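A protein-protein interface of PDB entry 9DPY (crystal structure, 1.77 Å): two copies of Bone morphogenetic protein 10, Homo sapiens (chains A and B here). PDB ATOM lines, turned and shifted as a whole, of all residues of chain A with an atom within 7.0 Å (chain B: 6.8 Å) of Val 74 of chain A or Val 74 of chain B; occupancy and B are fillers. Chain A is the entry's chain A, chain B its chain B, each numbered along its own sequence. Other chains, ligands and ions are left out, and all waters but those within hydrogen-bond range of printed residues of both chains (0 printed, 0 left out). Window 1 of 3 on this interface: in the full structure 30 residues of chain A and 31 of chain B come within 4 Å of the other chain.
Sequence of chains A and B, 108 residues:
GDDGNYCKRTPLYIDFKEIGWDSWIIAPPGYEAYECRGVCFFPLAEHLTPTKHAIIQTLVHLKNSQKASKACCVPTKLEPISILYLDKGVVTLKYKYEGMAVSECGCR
The side-chain sulfur (SG) of Cys 72 of chain A forms a disulfide with the side-chain sulfur (SG) of Cys 72 of chain B (2.0 Å).
O of Cys 72 of chain A sits at hydrogen-bond distance from N of Arg 108 of chain A (2.9 Å). The backbone NH (N) of Gly 106 of chain A sits at hydrogen-bond distance from the backbone carbonyl oxygen (O) of Val 74 of chain A (2.9 Å). The side-chain sulfur of Cys 36 of chain A is disulfide-bonded to the side-chain sulfur of Cys 105 of chain A (2.0 Å). The side-chain sulfur (SG) of Cys 40 of chain A forms a disulfide with the side-chain sulfur (SG) of Cys 107 of chain A, 2.1 Å away. SG of Cys 7 of chain B forms a disulfide with SG of Cys 73 of chain B, at 2.0 Å. The side-chain sulfur (SG) of Cys 36 of chain B forms a disulfide with the side-chain sulfur (SG) of Cys 105 of chain B (2.0 Å).
Among the printed residues, merely in contact across the chains: Pro 75 of chain A with Arg 108 of chain B, Arg 108 of chain A with Pro 75 of chain B, Cys 72 of chain A with Val 74 of chain B, Val 74 of chain A with Cys 72 of chain B, Val 74 of chain A with Val 74 of chain B and Val 74 of chain A with Arg 108 of chain B.
Of the printed residues of chain B, Cys 72 of chain A touches Cys 72 (2.0 Å) and Val 74 (3.6 Å). Of the printed residues of chain B, Pro 75 of chain A touches Arg 108. Printed residues of chain A within 4 Å of Cys 72 of chain B: Cys 72 and Val 74. Of the printed residues of chain A, Val 74 of chain B touches Cys 72 and Val 74. Of the printed residues of chain A, Arg 108 of chain B touches Val 74 and Pro 75.
Hydrophobic or aromatic side chains of chain A that line the printed part of chain B: Val 74 and Pro 75. Of the 17 printed residues of chain B, 4 touch a printed residue of chain A. Hydrophobic or aromatic side chains of chain B within 4 Å of the printed part of chain A: Val 74 and Pro 75. Among the printed residues, no Asp or Glu carboxylate lies within 4 Å of a Lys or Arg side-chain nitrogen of the other chain.
Cys 72 of chain B touches its own counterpart, Cys 72 of chain A. Cys 72 of chain A touches Val 74 of chain B, and with the chains exchanged Val 74 of chain A touches Cys 72 of chain B. Val 74 of chain A touches Arg 108 of chain B, but with the chains exchanged Arg 108 of chain A does not touch Val 74 of chain B (4.1 Å). Pro 75 of chain A touches Arg 108 of chain B, and with the chains exchanged Arg 108 of chain A touches Pro 75 of chain B. Positions printed for both chains: 7, 36, 37, 40, 71, 72, 73, 74, 75, 76, 77, 102, 104, 105, 106, 107 and 108.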
ATOM      1  N   CYS A   7      18.316   6.693  23.765  1.00  0.00           N
ATOM      2  CA  CYS A   7      19.658   7.037  23.315  1.00  0.00           C
ATOM      3  C   CYS A   7      20.077   8.425  23.793  1.00  0.00           C
ATOM      4  O   CYS A   7      19.389   9.412  23.540  1.00  0.00           O
ATOM      5  CB  CYS A   7      19.691   6.960  21.781  1.00  0.00           C
ATOM      6  SG  CYS A   7      21.316   7.390  21.016  1.00  0.00           S
ATOM      7  N   CYS A  36      27.715   6.646  24.305  1.00  0.00           N
ATOM      8  CA  CYS A  36      26.327   6.754  23.886  1.00  0.00           C
ATOM      9  C   CYS A  36      25.614   5.472  24.266  1.00  0.00           C
ATOM     10  O   CYS A  36      26.057   4.385  23.886  1.00  0.00           O
ATOM     11  CB  CYS A  36      26.206   6.983  22.387  1.00  0.00           C
ATOM     12  SG  CYS A  36      26.977   8.517  21.792  1.00  0.00           S
ATOM     13  N   ARG A  37      24.507   5.607  24.989  1.00  0.00           N
ATOM     14  CA  ARG A  37      23.797   4.471  25.550  1.00  0.00           C
ATOM     15  C   ARG A  37      22.297   4.710  25.469  1.00  0.00           C
ATOM     16  O   ARG A  37      21.833   5.841  25.612  1.00  0.00           O
ATOM     17  CB  ARG A  37      24.186   4.230  27.016  1.00  0.00           C
ATOM     18  CG  ARG A  37      25.603   3.771  27.205  1.00  0.00           C
ATOM     19  CD  ARG A  37      25.794   3.322  28.632  1.00  0.00           C
ATOM     20  NE  ARG A  37      25.113   2.059  28.872  1.00  0.00           N
ATOM     21  CZ  ARG A  37      25.706   0.876  28.810  1.00  0.00           C
ATOM     22  NH1 ARG A  37      26.987   0.760  28.496  1.00  0.00           N
ATOM     23  NH2 ARG A  37      25.001  -0.218  29.075  1.00  0.00           N
ATOM     24  N   GLY A  38      21.537   3.631  25.306  1.00  0.00           N
ATOM     25  CA  GLY A  38      20.086   3.711  25.232  1.00  0.00           C
ATOM     26  C   GLY A  38      19.551   3.196  23.906  1.00  0.00           C
ATOM     27  O   GLY A  38      20.298   2.863  22.988  1.00  0.00           O
ATOM     28  N   CYS A  40      16.978   3.154  20.426  1.00  0.00           N
ATOM     29  CA  CYS A  40      16.470   3.985  19.339  1.00  0.00           C
ATOM     30  C   CYS A  40      15.036   3.545  19.075  1.00  0.00           C
ATOM     31  O   CYS A  40      14.791   2.585  18.340  1.00  0.00           O
ATOM     32  CB  CYS A  40      17.345   3.846  18.106  1.00  0.00           C
ATOM     33  SG  CYS A  40      19.007   4.549  18.425  1.00  0.00           S
ATOM     34  N   ALA A  71      17.755   0.398  15.158  1.00  0.00           N
ATOM     35  CA  ALA A  71      18.889   1.287  14.897  1.00  0.00           C
ATOM     36  C   ALA A  71      19.738   1.415  16.156  1.00  0.00           C
ATOM     37  O   ALA A  71      19.258   1.223  17.278  1.00  0.00           O
ATOM     38  CB  ALA A  71      18.416   2.674  14.431  1.00  0.00           C
ATOM     39  N   CYS A  72      21.014   1.731  15.971  1.00  0.00           N
ATOM     40  CA  CYS A  72      21.972   1.706  17.066  1.00  0.00           C
ATOM     41  C   CYS A  72      22.314   3.122  17.513  1.00  0.00           C
ATOM     42  O   CYS A  72      22.409   4.042  16.696  1.00  0.00           O
ATOM     43  CB  CYS A  72      23.247   0.968  16.666  1.00  0.00           C
ATOM     44  SG  CYS A  72      24.137   0.343  18.139  1.00  0.00           S
ATOM     45  N   CYS A  73      22.466   3.282  18.822  1.00  0.00           N
ATOM     46  CA  CYS A  73      22.863   4.533  19.457  1.00  0.00           C
ATOM     47  C   CYS A  73      24.383   4.631  19.396  1.00  0.00           C
ATOM     48  O   CYS A  73      25.076   3.849  20.054  1.00  0.00           O
ATOM     49  CB  CYS A  73      22.355   4.530  20.897  1.00  0.00           C
ATOM     50  SG  CYS A  73      22.612   6.065  21.843  1.00  0.00           S
ATOM     51  N   VAL A  74      24.908   5.563  18.603  1.00  0.00           N
ATOM     52  CA  VAL A  74      26.351   5.665  18.374  1.00  0.00           C
ATOM     53  C   VAL A  74      26.787   7.123  18.421  1.00  0.00           C
ATOM     54  O   VAL A  74      25.977   8.044  18.245  1.00  0.00           O
ATOM     55  CB  VAL A  74      26.764   5.049  17.021  1.00  0.00           C
ATOM     56  CG1 VAL A  74      26.579   3.539  17.044  1.00  0.00           C
ATOM     57  CG2 VAL A  74      25.952   5.671  15.869  1.00  0.00           C
ATOM     58  N   PRO A  75      28.084   7.365  18.623  1.00  0.00           N
ATOM     59  CA  PRO A  75      28.591   8.737  18.488  1.00  0.00           C
ATOM     60  C   PRO A  75      28.430   9.246  17.066  1.00  0.00           C
ATOM     61  O   PRO A  75      28.782   8.567  16.097  1.00  0.00           O
ATOM     62  CB  PRO A  75      30.072   8.621  18.875  1.00  0.00           C
ATOM     63  CG  PRO A  75      30.162   7.381  19.684  1.00  0.00           C
ATOM     64  CD  PRO A  75      29.121   6.440  19.109  1.00  0.00           C
ATOM     65  N   THR A  76      27.911  10.464  16.953  1.00  0.00           N
ATOM     66  CA  THR A  76      27.808  11.152  15.680  1.00  0.00           C
ATOM     67  C   THR A  76      28.685  12.394  15.596  1.00  0.00           C
ATOM     68  O   THR A  76      28.764  13.014  14.529  1.00  0.00           O
ATOM     69  CB  THR A  76      26.351  11.559  15.431  1.00  0.00           C
ATOM     70  OG1 THR A  76      25.889  12.316  16.560  1.00  0.00           O
ATOM     71  CG2 THR A  76      25.469  10.328  15.243  1.00  0.00           C
ATOM     72  N   LYS A  77      29.315  12.798  16.693  1.00  0.00           N
ATOM     73  CA  LYS A  77      30.300  13.869  16.641  1.00  0.00           C
ATOM     74  C   LYS A  77      31.318  13.607  17.736  1.00  0.00           C
ATOM     75  O   LYS A  77      30.936  13.371  18.884  1.00  0.00           O
ATOM     76  CB  LYS A  77      29.666  15.253  16.819  1.00  0.00           C
ATOM     77  CG  LYS A  77      30.635  16.402  16.490  1.00  0.00           C
ATOM     78  CD  LYS A  77      29.944  17.764  16.575  1.00  0.00           C
ATOM     79  CE  LYS A  77      30.711  18.838  15.799  1.00  0.00           C
ATOM     80  NZ  LYS A  77      32.132  18.930  16.226  1.00  0.00           N
ATOM     81  N   VAL A 102      33.089  11.919  22.991  1.00  0.00           N
ATOM     82  CA  VAL A 102      31.784  12.074  22.356  1.00  0.00           C
ATOM     83  C   VAL A 102      31.214  13.440  22.687  1.00  0.00           C
ATOM     84  O   VAL A 102      31.110  13.818  23.861  1.00  0.00           O
ATOM     85  CB  VAL A 102      30.811  10.979  22.814  1.00  0.00           C
ATOM     86  CG1 VAL A 102      29.415  11.233  22.195  1.00  0.00           C
ATOM     87  CG2 VAL A 102      31.354   9.605  22.479  1.00  0.00           C
ATOM     88  N   GLU A 104      28.247  14.371  20.518  1.00  0.00           N
ATOM     89  CA  GLU A 104      26.864  14.122  20.133  1.00  0.00           C
ATOM     90  C   GLU A 104      26.640  12.643  19.868  1.00  0.00           C
ATOM     91  O   GLU A 104      27.518  11.959  19.335  1.00  0.00           O
ATOM     92  CB  GLU A 104      26.454  14.885  18.867  1.00  0.00           C
ATOM     93  CG  GLU A 104      26.832  16.368  18.923  1.00  0.00           C
ATOM     94  CD  GLU A 104      26.412  17.143  17.688  1.00  0.00           C
ATOM     95  OE1 GLU A 104      26.040  16.522  16.665  1.00  0.00           O
ATOM     96  OE2 GLU A 104      26.472  18.385  17.738  1.00  0.00           O
ATOM     97  N   CYS A 105      25.429  12.176  20.196  1.00  0.00           N
ATOM     98  CA  CYS A 105      24.957  10.823  19.926  1.00  0.00           C
ATOM     99  C   CYS A 105      23.808  10.860  18.927  1.00  0.00           C
ATOM    100  O   CYS A 105      23.064  11.840  18.851  1.00  0.00           O
ATOM    101  CB  CYS A 105      24.445  10.124  21.194  1.00  0.00           C
ATOM    102  SG  CYS A 105      25.713   9.956  22.484  1.00  0.00           S
ATOM    103  N   GLY A 106      23.626   9.759  18.204  1.00  0.00           N
ATOM    104  CA  GLY A 106      22.527   9.685  17.255  1.00  0.00           C
ATOM    105  C   GLY A 106      22.168   8.242  16.986  1.00  0.00           C
ATOM    106  O   GLY A 106      22.841   7.319  17.451  1.00  0.00           O
ATOM    107  N   CYS A 107      21.080   8.052  16.236  1.00  0.00           N
ATOM    108  CA  CYS A 107      20.619   6.723  15.852  1.00  0.00           C
ATOM    109  C   CYS A 107      20.992   6.451  14.399  1.00  0.00           C
ATOM    110  O   CYS A 107      20.652   7.236  13.500  1.00  0.00           O
ATOM    111  CB  CYS A 107      19.104   6.580  16.052  1.00  0.00           C
ATOM    112  SG  CYS A 107      18.673   6.496  17.850  1.00  0.00           S
ATOM    113  N   ARG A 108      21.666   5.327  14.175  1.00  0.00           N
ATOM    114  CA  ARG A 108      22.151   4.988  12.845  1.00  0.00           C
ATOM    115  C   ARG A 108      21.910   3.525  12.438  1.00  0.00           C
ATOM    116  O   ARG A 108      21.791   3.261  11.239  1.00  0.00           O
ATOM    117  CB  ARG A 108      23.657   5.300  12.758  1.00  0.00           C
ATOM    118  CG  ARG A 108      24.022   6.809  12.906  1.00  0.00           C
ATOM    119  CD  ARG A 108      23.555   7.624  11.683  1.00  0.00           C
ATOM    120  NE  ARG A 108      23.967   9.026  11.745  1.00  0.00           N
ATOM    121  CZ  ARG A 108      23.358   9.964  12.464  1.00  0.00           C
ATOM    122  NH1 ARG A 108      22.370   9.666  13.292  1.00  0.00           N
ATOM    123  NH2 ARG A 108      23.747  11.236  12.349  1.00  0.00           N
ATOM    124  OXT ARG A 108      21.815   2.579  13.240  1.00  0.00           O
ATOM    125  N   CYS B   7      31.170  -8.026  12.188  1.00  0.00           N
ATOM    126  CA  CYS B   7      30.436  -6.924  11.566  1.00  0.00           C
ATOM    127  C   CYS B   7      30.597  -6.921  10.051  1.00  0.00           C
ATOM    128  O   CYS B   7      31.718  -6.929   9.534  1.00  0.00           O
ATOM    129  CB  CYS B   7      30.922  -5.589  12.166  1.00  0.00           C
ATOM    130  SG  CYS B   7      30.239  -4.011  11.413  1.00  0.00           S
ATOM    131  N   CYS B  36      23.582  -3.757   8.466  1.00  0.00           N
ATOM    132  CA  CYS B  36      24.883  -4.020   9.079  1.00  0.00           C
ATOM    133  C   CYS B  36      24.647  -4.877  10.313  1.00  0.00           C
ATOM    134  O   CYS B  36      23.889  -4.479  11.204  1.00  0.00           O
ATOM    135  CB  CYS B  36      25.590  -2.722   9.458  1.00  0.00           C
ATOM    136  SG  CYS B  36      25.955  -1.671   8.049  1.00  0.00           S
ATOM    137  N   ARG B  37      25.261  -6.058  10.358  1.00  0.00           N
ATOM    138  CA  ARG B  37      25.068  -6.951  11.489  1.00  0.00           C
ATOM    139  C   ARG B  37      26.407  -7.568  11.853  1.00  0.00           C
ATOM    140  O   ARG B  37      27.301  -7.684  11.012  1.00  0.00           O
ATOM    141  CB  ARG B  37      24.073  -8.101  11.223  1.00  0.00           C
ATOM    142  CG  ARG B  37      22.719  -7.638  10.650  1.00  0.00           C
ATOM    143  CD  ARG B  37      21.829  -8.836  10.390  1.00  0.00           C
ATOM    144  NE  ARG B  37      21.507  -9.533  11.628  1.00  0.00           N
ATOM    145  CZ  ARG B  37      20.492  -9.215  12.421  1.00  0.00           C
ATOM    146  NH1 ARG B  37      19.657  -8.236  12.115  1.00  0.00           N
ATOM    147  NH2 ARG B  37      20.317  -9.890  13.555  1.00  0.00           N
ATOM    148  N   CYS B  40      31.708  -6.214  16.817  1.00  0.00           N
ATOM    149  CA  CYS B  40      32.923  -5.416  16.670  1.00  0.00           C
ATOM    150  C   CYS B  40      33.925  -5.963  17.672  1.00  0.00           C
ATOM    151  O   CYS B  40      33.860  -5.655  18.866  1.00  0.00           O
ATOM    152  CB  CYS B  40      32.621  -3.943  16.895  1.00  0.00           C
ATOM    153  SG  CYS B  40      31.574  -3.274  15.518  1.00  0.00           S
ATOM    154  N   ALA B  71      31.686  -1.526  20.715  1.00  0.00           N
ATOM    155  CA  ALA B  71      31.361  -0.663  19.592  1.00  0.00           C
ATOM    156  C   ALA B  71      30.221  -1.288  18.790  1.00  0.00           C
ATOM    157  O   ALA B  71      30.003  -2.500  18.817  1.00  0.00           O
ATOM    158  CB  ALA B  71      32.582  -0.450  18.694  1.00  0.00           C
ATOM    159  N   CYS B  72      29.489  -0.455  18.063  1.00  0.00           N
ATOM    160  CA  CYS B  72      28.318  -0.924  17.339  1.00  0.00           C
ATOM    161  C   CYS B  72      28.593  -1.008  15.842  1.00  0.00           C
ATOM    162  O   CYS B  72      29.207  -0.111  15.261  1.00  0.00           O
ATOM    163  CB  CYS B  72      27.116  -0.015  17.602  1.00  0.00           C
ATOM    164  SG  CYS B  72      25.542  -0.904  17.376  1.00  0.00           S
ATOM    165  N   CYS B  73      28.100  -2.079  15.218  1.00  0.00           N
ATOM    166  CA  CYS B  73      28.158  -2.259  13.766  1.00  0.00           C
ATOM    167  C   CYS B  73      27.047  -1.446  13.115  1.00  0.00           C
ATOM    168  O   CYS B  73      25.871  -1.809  13.231  1.00  0.00           O
ATOM    169  CB  CYS B  73      27.975  -3.730  13.403  1.00  0.00           C
ATOM    170  SG  CYS B  73      28.232  -4.113  11.637  1.00  0.00           S
ATOM    171  N   VAL B  74      27.402  -0.389  12.390  1.00  0.00           N
ATOM    172  CA  VAL B  74      26.406   0.524  11.823  1.00  0.00           C
ATOM    173  C   VAL B  74      26.785   0.886  10.395  1.00  0.00           C
ATOM    174  O   VAL B  74      27.956   0.799   9.997  1.00  0.00           O
ATOM    175  CB  VAL B  74      26.264   1.812  12.656  1.00  0.00           C
ATOM    176  CG1 VAL B  74      25.653   1.507  14.014  1.00  0.00           C
ATOM    177  CG2 VAL B  74      27.632   2.504  12.805  1.00  0.00           C
ATOM    178  N   PRO B  75      25.814   1.358   9.612  1.00  0.00           N
ATOM    179  CA  PRO B  75      26.150   1.897   8.289  1.00  0.00           C
ATOM    180  C   PRO B  75      27.060   3.111   8.406  1.00  0.00           C
ATOM    181  O   PRO B  75      26.802   4.037   9.181  1.00  0.00           O
ATOM    182  CB  PRO B  75      24.784   2.269   7.689  1.00  0.00           C
ATOM    183  CG  PRO B  75      23.772   1.488   8.482  1.00  0.00           C
ATOM    184  CD  PRO B  75      24.364   1.402   9.878  1.00  0.00           C
ATOM    185  N   THR B  76      28.133   3.104   7.619  1.00  0.00           N
ATOM    186  CA  THR B  76      29.030   4.241   7.540  1.00  0.00           C
ATOM    187  C   THR B  76      28.977   4.948   6.195  1.00  0.00           C
ATOM    188  O   THR B  76      29.518   6.051   6.067  1.00  0.00           O
ATOM    189  CB  THR B  76      30.469   3.790   7.834  1.00  0.00           C
ATOM    190  OG1 THR B  76      30.817   2.701   6.970  1.00  0.00           O
ATOM    191  CG2 THR B  76      30.578   3.303   9.265  1.00  0.00           C
ATOM    192  N   LYS B  77      28.320   4.355   5.205  1.00  0.00           N
ATOM    193  CA  LYS B  77      28.148   4.956   3.890  1.00  0.00           C
ATOM    194  C   LYS B  77      26.790   4.500   3.366  1.00  0.00           C
ATOM    195  O   LYS B  77      26.487   3.303   3.394  1.00  0.00           O
ATOM    196  CB  LYS B  77      29.294   4.541   2.955  1.00  0.00           C
ATOM    197  CG  LYS B  77      29.396   5.353   1.652  1.00  0.00           C
ATOM    198  CD  LYS B  77      30.244   6.600   1.833  1.00  0.00           C
ATOM    199  CE  LYS B  77      30.450   7.321   0.512  1.00  0.00           C
ATOM    200  NZ  LYS B  77      29.172   7.851  -0.037  1.00  0.00           N
ATOM    201  N   VAL B 102      22.619   0.716   2.266  1.00  0.00           N
ATOM    202  CA  VAL B 102      23.971   0.643   2.827  1.00  0.00           C
ATOM    203  C   VAL B 102      24.955   0.230   1.744  1.00  0.00           C
ATOM    204  O   VAL B 102      24.786  -0.816   1.107  1.00  0.00           O
ATOM    205  CB  VAL B 102      24.050  -0.350   4.000  1.00  0.00           C
ATOM    206  CG1 VAL B 102      25.477  -0.291   4.683  1.00  0.00           C
ATOM    207  CG2 VAL B 102      22.956  -0.111   5.017  1.00  0.00           C
ATOM    208  N   GLU B 104      28.526   0.681   2.863  1.00  0.00           N
ATOM    209  CA  GLU B 104      29.608   0.276   3.755  1.00  0.00           C
ATOM    210  C   GLU B 104      29.160   0.269   5.211  1.00  0.00           C
ATOM    211  O   GLU B 104      28.346   1.097   5.632  1.00  0.00           O
ATOM    212  CB  GLU B 104      30.845   1.193   3.655  1.00  0.00           C
ATOM    213  CG  GLU B 104      31.435   1.250   2.271  1.00  0.00           C
ATOM    214  CD  GLU B 104      32.525   2.291   2.161  1.00  0.00           C
ATOM    215  OE1 GLU B 104      32.891   2.887   3.201  1.00  0.00           O
ATOM    216  OE2 GLU B 104      33.004   2.518   1.035  1.00  0.00           O
ATOM    217  N   CYS B 105      29.739  -0.662   5.980  1.00  0.00           N
ATOM    218  CA  CYS B 105      29.518  -0.816   7.414  1.00  0.00           C
ATOM    219  C   CYS B 105      30.816  -0.554   8.175  1.00  0.00           C
ATOM    220  O   CYS B 105      31.915  -0.749   7.649  1.00  0.00           O
ATOM    221  CB  CYS B 105      29.024  -2.236   7.774  1.00  0.00           C
ATOM    222  SG  CYS B 105      27.398  -2.676   7.007  1.00  0.00           S
ATOM    223  N   GLY B 106      30.684  -0.168   9.444  1.00  0.00           N
ATOM    224  CA  GLY B 106      31.853   0.116  10.264  1.00  0.00           C
ATOM    225  C   GLY B 106      31.517   0.039  11.737  1.00  0.00           C
ATOM    226  O   GLY B 106      30.350  -0.033  12.127  1.00  0.00           O
ATOM    227  N   CYS B 107      32.557   0.040  12.569  1.00  0.00           N
ATOM    228  CA  CYS B 107      32.386  -0.008  14.020  1.00  0.00           C
ATOM    229  C   CYS B 107      32.488   1.401  14.586  1.00  0.00           C
ATOM    230  O   CYS B 107      33.468   2.105  14.328  1.00  0.00           O
ATOM    231  CB  CYS B 107      33.416  -0.941  14.664  1.00  0.00           C
ATOM    232  SG  CYS B 107      33.014  -2.676  14.208  1.00  0.00           S
ATOM    233  N   ARG B 108      31.468   1.813  15.339  1.00  0.00           N
ATOM    234  CA  ARG B 108      31.404   3.185  15.836  1.00  0.00           C
ATOM    235  C   ARG B 108      31.018   3.294  17.313  1.00  0.00           C
ATOM    236  O   ARG B 108      31.452   4.237  17.993  1.00  0.00           O
ATOM    237  CB  ARG B 108      30.397   4.006  14.994  1.00  0.00           C
ATOM    238  CG  ARG B 108      30.802   4.205  13.527  1.00  0.00           C
ATOM    239  CD  ARG B 108      32.098   5.015  13.450  1.00  0.00           C
ATOM    240  NE  ARG B 108      32.420   5.416  12.082  1.00  0.00           N
ATOM    241  CZ  ARG B 108      33.107   4.659  11.236  1.00  0.00           C
ATOM    242  NH1 ARG B 108      33.508   3.438  11.570  1.00  0.00           N
ATOM    243  NH2 ARG B 108      33.395   5.141  10.027  1.00  0.00           N
ATOM    244  OXT ARG B 108      30.262   2.479  17.854  1.00  0.00           O
